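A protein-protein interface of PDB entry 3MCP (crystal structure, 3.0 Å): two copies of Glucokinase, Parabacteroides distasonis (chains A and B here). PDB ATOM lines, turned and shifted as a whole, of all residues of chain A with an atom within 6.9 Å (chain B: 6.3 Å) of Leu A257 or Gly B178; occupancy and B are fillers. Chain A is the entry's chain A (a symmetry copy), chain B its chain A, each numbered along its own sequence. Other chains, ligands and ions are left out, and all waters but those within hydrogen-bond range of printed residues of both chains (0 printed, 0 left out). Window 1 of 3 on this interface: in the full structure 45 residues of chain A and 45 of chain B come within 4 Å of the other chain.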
ATOM      1  N   ASN A 149      30.678 -18.139  36.191  1.00  0.00           N
ATOM      2  CA  ASN A 149      29.291 -18.479  35.846  1.00  0.00           C
ATOM      3  C   ASN A 149      28.957 -19.941  36.185  1.00  0.00           C
ATOM      4  O   ASN A 149      29.672 -20.859  35.772  1.00  0.00           O
ATOM      5  CB  ASN A 149      29.030 -18.209  34.359  1.00  0.00           C
ATOM      6  CG  ASN A 149      29.129 -16.715  34.002  1.00  0.00           C
ATOM      7  OD1 ASN A 149      29.371 -15.865  34.870  1.00  0.00           O
ATOM      8  ND2 ASN A 149      28.939 -16.398  32.720  1.00  0.00           N
ATOM      9  N   ILE A 165      25.512 -15.649  37.756  1.00  0.00           N
ATOM     10  CA  ILE A 165      26.509 -14.981  36.904  1.00  0.00           C
ATOM     11  C   ILE A 165      27.416 -14.097  37.760  1.00  0.00           C
ATOM     12  O   ILE A 165      27.005 -13.039  38.249  1.00  0.00           O
ATOM     13  CB  ILE A 165      25.855 -14.130  35.794  1.00  0.00           C
ATOM     14  CG1 ILE A 165      24.928 -14.991  34.942  1.00  0.00           C
ATOM     15  CG2 ILE A 165      26.913 -13.496  34.924  1.00  0.00           C
ATOM     16  CD1 ILE A 165      25.602 -16.182  34.325  1.00  0.00           C
ATOM     17  N   ALA A 252      23.423 -29.223  27.693  1.00  0.00           N
ATOM     18  CA  ALA A 252      24.215 -28.765  26.548  1.00  0.00           C
ATOM     19  C   ALA A 252      23.688 -27.455  25.992  1.00  0.00           C
ATOM     20  O   ALA A 252      24.417 -26.471  25.911  1.00  0.00           O
ATOM     21  CB  ALA A 252      24.226 -29.807  25.471  1.00  0.00           C
ATOM     22  N   SER A 253      22.414 -27.435  25.617  1.00  0.00           N
ATOM     23  CA  SER A 253      21.823 -26.237  25.007  1.00  0.00           C
ATOM     24  C   SER A 253      21.621 -25.099  26.014  1.00  0.00           C
ATOM     25  O   SER A 253      21.622 -23.933  25.640  1.00  0.00           O
ATOM     26  CB  SER A 253      20.509 -26.578  24.269  1.00  0.00           C
ATOM     27  OG  SER A 253      19.649 -27.362  25.061  1.00  0.00           O
ATOM     28  N   ALA A 254      21.493 -25.434  27.289  1.00  0.00           N
ATOM     29  CA  ALA A 254      21.360 -24.410  28.328  1.00  0.00           C
ATOM     30  C   ALA A 254      22.692 -23.745  28.569  1.00  0.00           C
ATOM     31  O   ALA A 254      22.783 -22.525  28.629  1.00  0.00           O
ATOM     32  CB  ALA A 254      20.847 -25.014  29.611  1.00  0.00           C
ATOM     33  N   ILE A 255      23.738 -24.553  28.685  1.00  0.00           N
ATOM     34  CA  ILE A 255      25.064 -24.036  29.003  1.00  0.00           C
ATOM     35  C   ILE A 255      25.673 -23.256  27.827  1.00  0.00           C
ATOM     36  O   ILE A 255      26.557 -22.420  28.024  1.00  0.00           O
ATOM     37  CB  ILE A 255      26.020 -25.168  29.437  1.00  0.00           C
ATOM     38  CG1 ILE A 255      27.074 -24.620  30.383  1.00  0.00           C
ATOM     39  CG2 ILE A 255      26.644 -25.842  28.225  1.00  0.00           C
ATOM     40  CD1 ILE A 255      26.481 -24.029  31.653  1.00  0.00           C
ATOM     41  N   THR A 256      25.193 -23.527  26.611  1.00  0.00           N
ATOM     42  CA  THR A 256      25.638 -22.786  25.431  1.00  0.00           C
ATOM     43  C   THR A 256      25.400 -21.288  25.593  1.00  0.00           C
ATOM     44  O   THR A 256      26.209 -20.482  25.147  1.00  0.00           O
ATOM     45  CB  THR A 256      24.934 -23.260  24.161  1.00  0.00           C
ATOM     46  OG1 THR A 256      25.366 -24.593  23.844  1.00  0.00           O
ATOM     47  CG2 THR A 256      25.253 -22.331  22.994  1.00  0.00           C
ATOM     48  N   LEU A 257      24.293 -20.917  26.234  1.00  0.00           N
ATOM     49  CA  LEU A 257      24.006 -19.498  26.498  1.00  0.00           C
ATOM     50  C   LEU A 257      24.760 -18.964  27.714  1.00  0.00           C
ATOM     51  O   LEU A 257      25.235 -17.830  27.696  1.00  0.00           O
ATOM     52  CB  LEU A 257      22.505 -19.252  26.689  1.00  0.00           C
ATOM     53  CG  LEU A 257      21.653 -19.274  25.424  1.00  0.00           C
ATOM     54  CD1 LEU A 257      21.352 -20.723  24.978  1.00  0.00           C
ATOM     55  CD2 LEU A 257      20.376 -18.517  25.657  1.00  0.00           C
ATOM     56  N   ILE A 258      24.862 -19.774  28.768  1.00  0.00           N
ATOM     57  CA  ILE A 258      25.520 -19.336  30.011  1.00  0.00           C
ATOM     58  C   ILE A 258      27.046 -19.370  29.906  1.00  0.00           C
ATOM     59  O   ILE A 258      27.726 -18.442  30.351  1.00  0.00           O
ATOM     60  CB  ILE A 258      25.108 -20.212  31.206  1.00  0.00           C
ATOM     61  CG1 ILE A 258      23.574 -20.241  31.363  1.00  0.00           C
ATOM     62  CG2 ILE A 258      25.794 -19.729  32.483  1.00  0.00           C
ATOM     63  CD1 ILE A 258      22.932 -18.881  31.442  1.00  0.00           C
ATOM     64  N   ASP A 259      27.574 -20.464  29.355  1.00  0.00           N
ATOM     65  CA  ASP A 259      29.011 -20.633  29.190  1.00  0.00           C
ATOM     66  C   ASP A 259      29.718 -20.593  30.552  1.00  0.00           C
ATOM     67  O   ASP A 259      30.545 -19.716  30.807  1.00  0.00           O
ATOM     68  CB  ASP A 259      29.570 -19.546  28.250  1.00  0.00           C
ATOM     69  CG  ASP A 259      31.070 -19.695  27.991  1.00  0.00           C
ATOM     70  OD1 ASP A 259      31.592 -20.828  28.094  1.00  0.00           O
ATOM     71  OD2 ASP A 259      31.724 -18.673  27.682  1.00  0.00           O
ATOM     72  N   GLY A 260      29.367 -21.537  31.426  1.00  0.00           N
ATOM     73  CA  GLY A 260      29.981 -21.631  32.759  1.00  0.00           C
ATOM     74  C   GLY A 260      30.017 -23.069  33.231  1.00  0.00           C
ATOM     75  O   GLY A 260      29.676 -23.967  32.480  1.00  0.00           O
ATOM     76  N   LEU B 151      17.838 -10.424  24.883  1.00  0.00           N
ATOM     77  CA  LEU B 151      18.529 -11.357  24.003  1.00  0.00           C
ATOM     78  C   LEU B 151      18.415 -10.822  22.582  1.00  0.00           C
ATOM     79  O   LEU B 151      17.346 -10.853  21.985  1.00  0.00           O
ATOM     80  CB  LEU B 151      17.899 -12.740  24.091  1.00  0.00           C
ATOM     81  CG  LEU B 151      18.295 -13.732  22.993  1.00  0.00           C
ATOM     82  CD1 LEU B 151      19.782 -13.963  22.986  1.00  0.00           C
ATOM     83  CD2 LEU B 151      17.551 -15.038  23.172  1.00  0.00           C
ATOM     84  N   GLY B 152      19.509 -10.281  22.065  1.00  0.00           N
ATOM     85  CA  GLY B 152      19.522  -9.727  20.717  1.00  0.00           C
ATOM     86  C   GLY B 152      20.138 -10.704  19.755  1.00  0.00           C
ATOM     87  O   GLY B 152      21.170 -11.278  20.041  1.00  0.00           O
ATOM     88  N   GLY B 160      23.897 -14.804  14.612  1.00  0.00           N
ATOM     89  CA  GLY B 160      24.628 -14.244  15.734  1.00  0.00           C
ATOM     90  C   GLY B 160      23.694 -13.804  16.825  1.00  0.00           C
ATOM     91  O   GLY B 160      22.502 -13.648  16.596  1.00  0.00           O
ATOM     92  N   ALA B 161      24.237 -13.600  18.020  1.00  0.00           N
ATOM     93  CA  ALA B 161      23.426 -13.205  19.161  1.00  0.00           C
ATOM     94  C   ALA B 161      24.262 -12.692  20.321  1.00  0.00           C
ATOM     95  O   ALA B 161      25.447 -12.999  20.433  1.00  0.00           O
ATOM     96  CB  ALA B 161      22.565 -14.377  19.617  1.00  0.00           C
ATOM     97  N   GLY B 162      23.624 -11.908  21.184  1.00  0.00           N
ATOM     98  CA  GLY B 162      24.257 -11.374  22.392  1.00  0.00           C
ATOM     99  C   GLY B 162      23.231 -11.308  23.508  1.00  0.00           C
ATOM    100  O   GLY B 162      22.032 -11.218  23.239  1.00  0.00           O
ATOM    101  N   VAL B 163      23.691 -11.366  24.757  1.00  0.00           N
ATOM    102  CA  VAL B 163      22.779 -11.338  25.895  1.00  0.00           C
ATOM    103  C   VAL B 163      23.196 -10.309  26.922  1.00  0.00           C
ATOM    104  O   VAL B 163      24.342 -10.307  27.381  1.00  0.00           O
ATOM    105  CB  VAL B 163      22.681 -12.725  26.580  1.00  0.00           C
ATOM    106  CG1 VAL B 163      22.025 -12.607  27.952  1.00  0.00           C
ATOM    107  CG2 VAL B 163      21.919 -13.697  25.704  1.00  0.00           C
ATOM    108  N   LEU B 170      26.532 -10.430  29.018  1.00  0.00           N
ATOM    109  CA  LEU B 170      26.834 -11.794  29.454  1.00  0.00           C
ATOM    110  C   LEU B 170      27.998 -12.365  28.631  1.00  0.00           C
ATOM    111  O   LEU B 170      27.797 -12.992  27.585  1.00  0.00           O
ATOM    112  CB  LEU B 170      25.602 -12.685  29.347  1.00  0.00           C
ATOM    113  CG  LEU B 170      25.676 -13.928  30.233  1.00  0.00           C
ATOM    114  CD1 LEU B 170      24.363 -14.692  30.221  1.00  0.00           C
ATOM    115  CD2 LEU B 170      26.815 -14.804  29.802  1.00  0.00           C
ATOM    116  N   ARG B 171      29.213 -12.161  29.140  1.00  0.00           N
ATOM    117  CA  ARG B 171      30.446 -12.534  28.433  1.00  0.00           C
ATOM    118  C   ARG B 171      30.679 -14.035  28.365  1.00  0.00           C
ATOM    119  O   ARG B 171      31.085 -14.561  27.329  1.00  0.00           O
ATOM    120  CB  ARG B 171      31.656 -11.888  29.116  1.00  0.00           C
ATOM    121  CG  ARG B 171      31.618 -10.377  29.155  1.00  0.00           C
ATOM    122  CD  ARG B 171      33.006  -9.789  29.468  1.00  0.00           C
ATOM    123  NE  ARG B 171      33.232  -8.536  28.747  1.00  0.00           N
ATOM    124  CZ  ARG B 171      33.385  -8.452  27.421  1.00  0.00           C
ATOM    125  NH1 ARG B 171      33.301  -9.543  26.651  1.00  0.00           N
ATOM    126  NH2 ARG B 171      33.591  -7.275  26.856  1.00  0.00           N
ATOM    127  N   GLY B 172      30.477 -14.710  29.486  1.00  0.00           N
ATOM    128  CA  GLY B 172      30.725 -16.136  29.561  1.00  0.00           C
ATOM    129  C   GLY B 172      32.153 -16.385  29.954  1.00  0.00           C
ATOM    130  O   GLY B 172      33.016 -15.558  29.711  1.00  0.00           O
ATOM    131  N   ALA B 176      32.305 -16.826  25.338  1.00  0.00           N
ATOM    132  CA  ALA B 176      31.375 -17.473  24.425  1.00  0.00           C
ATOM    133  C   ALA B 176      29.954 -17.439  24.963  1.00  0.00           C
ATOM    134  O   ALA B 176      29.138 -18.310  24.654  1.00  0.00           O
ATOM    135  CB  ALA B 176      31.808 -18.921  24.176  1.00  0.00           C
ATOM    136  N   GLY B 177      29.652 -16.437  25.767  1.00  0.00           N
ATOM    137  CA  GLY B 177      28.325 -16.304  26.309  1.00  0.00           C
ATOM    138  C   GLY B 177      27.335 -15.909  25.233  1.00  0.00           C
ATOM    139  O   GLY B 177      27.710 -15.290  24.234  1.00  0.00           O
ATOM    140  N   GLY B 178      26.083 -16.322  25.416  1.00  0.00           N
ATOM    141  CA  GLY B 178      24.996 -15.938  24.530  1.00  0.00           C
ATOM    142  C   GLY B 178      25.022 -16.507  23.121  1.00  0.00           C
ATOM    143  O   GLY B 178      24.382 -15.963  22.237  1.00  0.00           O
ATOM    144  N   TYR B 179      25.766 -17.586  22.893  1.00  0.00           N
ATOM    145  CA  TYR B 179      25.753 -18.232  21.572  1.00  0.00           C
ATOM    146  C   TYR B 179      24.413 -18.939  21.361  1.00  0.00           C
ATOM    147  O   TYR B 179      23.927 -19.612  22.262  1.00  0.00           O
ATOM    148  CB  TYR B 179      26.884 -19.280  21.428  1.00  0.00           C
ATOM    149  CG  TYR B 179      28.303 -18.742  21.186  1.00  0.00           C
ATOM    150  CD1 TYR B 179      28.528 -17.418  20.786  1.00  0.00           C
ATOM    151  CD2 TYR B 179      29.406 -19.610  21.227  1.00  0.00           C
ATOM    152  CE1 TYR B 179      29.827 -16.951  20.530  1.00  0.00           C
ATOM    153  CE2 TYR B 179      30.702 -19.156  20.957  1.00  0.00           C
ATOM    154  CZ  TYR B 179      30.906 -17.828  20.610  1.00  0.00           C
ATOM    155  OH  TYR B 179      32.187 -17.372  20.342  1.00  0.00           O
ATOM    156  N   VAL B 180      23.804 -18.757  20.188  1.00  0.00           N
ATOM    157  CA  VAL B 180      22.582 -19.505  19.840  1.00  0.00           C
ATOM    158  C   VAL B 180      22.721 -20.216  18.512  1.00  0.00           C
ATOM    159  O   VAL B 180      21.867 -21.018  18.151  1.00  0.00           O
ATOM    160  CB  VAL B 180      21.335 -18.603  19.747  1.00  0.00           C
ATOM    161  CG1 VAL B 180      20.992 -18.033  21.099  1.00  0.00           C
ATOM    162  CG2 VAL B 180      21.545 -17.502  18.700  1.00  0.00           C
ATOM    163  N   TRP B 181      23.799 -19.930  17.789  1.00  0.00           N
ATOM    164  CA  TRP B 181      24.001 -20.482  16.446  1.00  0.00           C
ATOM    165  C   TRP B 181      24.249 -21.974  16.434  1.00  0.00           C
ATOM    166  O   TRP B 181      23.945 -22.644  15.457  1.00  0.00           O
ATOM    167  CB  TRP B 181      25.171 -19.779  15.751  1.00  0.00           C
ATOM    168  CG  TRP B 181      26.498 -20.042  16.385  1.00  0.00           C
ATOM    169  CD1 TRP B 181      27.040 -19.384  17.445  1.00  0.00           C
ATOM    170  CD2 TRP B 181      27.456 -21.022  15.989  1.00  0.00           C
ATOM    171  NE1 TRP B 181      28.272 -19.897  17.741  1.00  0.00           N
ATOM    172  CE2 TRP B 181      28.554 -20.906  16.862  1.00  0.00           C
ATOM    173  CE3 TRP B 181      27.493 -21.993  14.979  1.00  0.00           C
ATOM    174  CZ2 TRP B 181      29.683 -21.723  16.760  1.00  0.00           C
ATOM    175  CZ3 TRP B 181      28.611 -22.802  14.879  1.00  0.00           C
ATOM    176  CH2 TRP B 181      29.695 -22.660  15.767  1.00  0.00           C
ATOM    177  N   LEU B 183      23.019 -24.249  18.617  1.00  0.00           N
ATOM    178  CA  LEU B 183      21.995 -25.060  19.275  1.00  0.00           C
ATOM    179  C   LEU B 183      21.540 -26.125  18.289  1.00  0.00           C
ATOM    180  O   LEU B 183      21.768 -25.995  17.073  1.00  0.00           O
ATOM    181  CB  LEU B 183      20.804 -24.202  19.722  1.00  0.00           C
ATOM    182  CG  LEU B 183      21.030 -23.229  20.891  1.00  0.00           C
ATOM    183  CD1 LEU B 183      19.850 -22.293  21.049  1.00  0.00           C
ATOM    184  CD2 LEU B 183      21.267 -23.979  22.157  1.00  0.00           C
ATOM    185  N   SER B 253      13.987 -22.004  23.493  1.00  0.00           N
ATOM    186  CA  SER B 253      14.809 -22.688  24.499  1.00  0.00           C
ATOM    187  C   SER B 253      15.925 -21.797  25.056  1.00  0.00           C
ATOM    188  O   SER B 253      16.363 -21.985  26.184  1.00  0.00           O
ATOM    189  CB  SER B 253      15.371 -24.018  23.948  1.00  0.00           C
ATOM    190  OG  SER B 253      15.950 -23.858  22.675  1.00  0.00           O
ATOM    191  N   ALA B 254      16.348 -20.805  24.288  1.00  0.00           N
ATOM    192  CA  ALA B 254      17.366 -19.864  24.763  1.00  0.00           C
ATOM    193  C   ALA B 254      16.760 -18.915  25.767  1.00  0.00           C
ATOM    194  O   ALA B 254      17.324 -18.680  26.829  1.00  0.00           O
ATOM    195  CB  ALA B 254      17.956 -19.088  23.613  1.00  0.00           C
ATOM    196  N   ILE B 255      15.590 -18.383  25.438  1.00  0.00           N
ATOM    197  CA  ILE B 255      14.945 -17.387  26.286  1.00  0.00           C
ATOM    198  C   ILE B 255      14.409 -18.003  27.589  1.00  0.00           C
ATOM    199  O   ILE B 255      14.220 -17.297  28.581  1.00  0.00           O
ATOM    200  CB  ILE B 255      13.805 -16.664  25.538  1.00  0.00           C
ATOM    201  CG1 ILE B 255      13.628 -15.262  26.094  1.00  0.00           C
ATOM    202  CG2 ILE B 255      12.516 -17.467  25.610  1.00  0.00           C
ATOM    203  CD1 ILE B 255      14.874 -14.402  25.943  1.00  0.00           C
ATOM    204  N   LEU B 257      16.035 -19.797  29.602  1.00  0.00           N
ATOM    205  CA  LEU B 257      17.070 -19.554  30.619  1.00  0.00           C
ATOM    206  C   LEU B 257      17.223 -18.073  30.958  1.00  0.00           C
ATOM    207  O   LEU B 257      17.417 -17.722  32.120  1.00  0.00           O
ATOM    208  CB  LEU B 257      18.430 -20.114  30.187  1.00  0.00           C
ATOM    209  CG  LEU B 257      18.590 -21.629  30.267  1.00  0.00           C
ATOM    210  CD1 LEU B 257      17.926 -22.326  29.058  1.00  0.00           C
ATOM    211  CD2 LEU B 257      20.049 -21.983  30.344  1.00  0.00           C
ATOM    212  N   ILE B 258      17.145 -17.209  29.945  1.00  0.00           N
ATOM    213  CA  ILE B 258      17.336 -15.763  30.154  1.00  0.00           C
ATOM    214  C   ILE B 258      16.096 -15.092  30.750  1.00  0.00           C
ATOM    215  O   ILE B 258      16.205 -14.265  31.658  1.00  0.00           O
ATOM    216  CB  ILE B 258      17.677 -15.043  28.839  1.00  0.00           C
ATOM    217  CG1 ILE B 258      18.911 -15.680  28.169  1.00  0.00           C
ATOM    218  CG2 ILE B 258      17.881 -13.549  29.087  1.00  0.00           C
ATOM    219  CD1 ILE B 258      20.120 -15.780  29.061  1.00  0.00           C
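The backbone NH of Ala B176 lies within hydrogen-bond range of the side-chain carboxylate of Asp A259, 3.0 Å away. The backbone NH (N) of Gly B178 sits at hydrogen-bond distance from the backbone carbonyl oxygen (O) of Leu A257, 2.9 Å away.
Ala A254 touches Leu B257, and with the chains exchanged Leu A257 touches Ala B254. Of the 15 pairs that touch across the chains among the printed residues, 2 have their exchanged pair printed and touching as well.
Gly B172 touches Asn A149. Leu B183 touches Ser A253 (CD2 to CB, 3.4 Å). Tyr B179 touches Thr A256. O of Leu A257 touches CA of Gly B177 (3.7 Å). Tyr B179 touches Leu A257. Leu A257 touches Ala B254. CD2 of Leu B170 touches O of Ile A258 (3.8 Å). Ile A258 touches Gly B172 (O to CA, 3.9 Å). Asp A259 touches Gly B172. Asp A259 touches Gly B177.
Printed residues of chain B within 4 Å of Asn A149: Leu B170 and Gly B172. Printed residues of chain B within 4 Å of Leu A257: Gly B177, Gly B178, Tyr B179 and Ala B254. Of the printed residues of chain B, Ile A258 touches Leu B170 (3.8 Å) and Gly B172 (3.9 Å). Of the printed residues of chain B, Asp A259 touches Gly B172, Ala B176 and Gly B177. Gly B160 touches none of the printed residues of chain A. Gly B178 touches just one residue of chain A: Leu A257. Of the printed residues of chain A, Ala B254 touches Leu A257. Of the printed residues of chain A, Leu B257 touches Ala A254. The nearest printed residue of chain B that does not touch Leu A257 is Leu B170 (4.01 Å).
The backbone carbonyl oxygen (O) of Val B163 sits at hydrogen-bond distance from the backbone NH (N) of Leu B170 (2.7 Å). The backbone NH of Ala B176 sits at hydrogen-bond distance from the backbone carbonyl oxygen of Arg B171 (3.3 Å). The backbone carbonyl oxygen of Arg B171 is in hydrogen-bond range of the backbone NH of Gly B177. The side-chain amide nitrogen (ND2) of Asn A149 sits at hydrogen-bond distance from the backbone carbonyl oxygen (O) of Ile A258 (3.4 Å). O of Ala A252 lies within hydrogen-bond range of OG1 of Thr A256 (2.9 Å).
Hydrophobic or aromatic side chains of chain B within 4 Å of the printed part of chain A: Leu B170, Ala B176, Tyr B179, Leu B183, Ala B254 and Leu B257. Hydrophobic or aromatic side chains of chain A that line the printed part of chain B: Ala A254 and Leu A257. Along chain A the printed residues that touch a printed residue of chain B span positions 149 to 259. Among the printed residues, no Asp or Glu carboxylate lies within 4 Å of a Lys or Arg side-chain nitrogen of the other chain.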
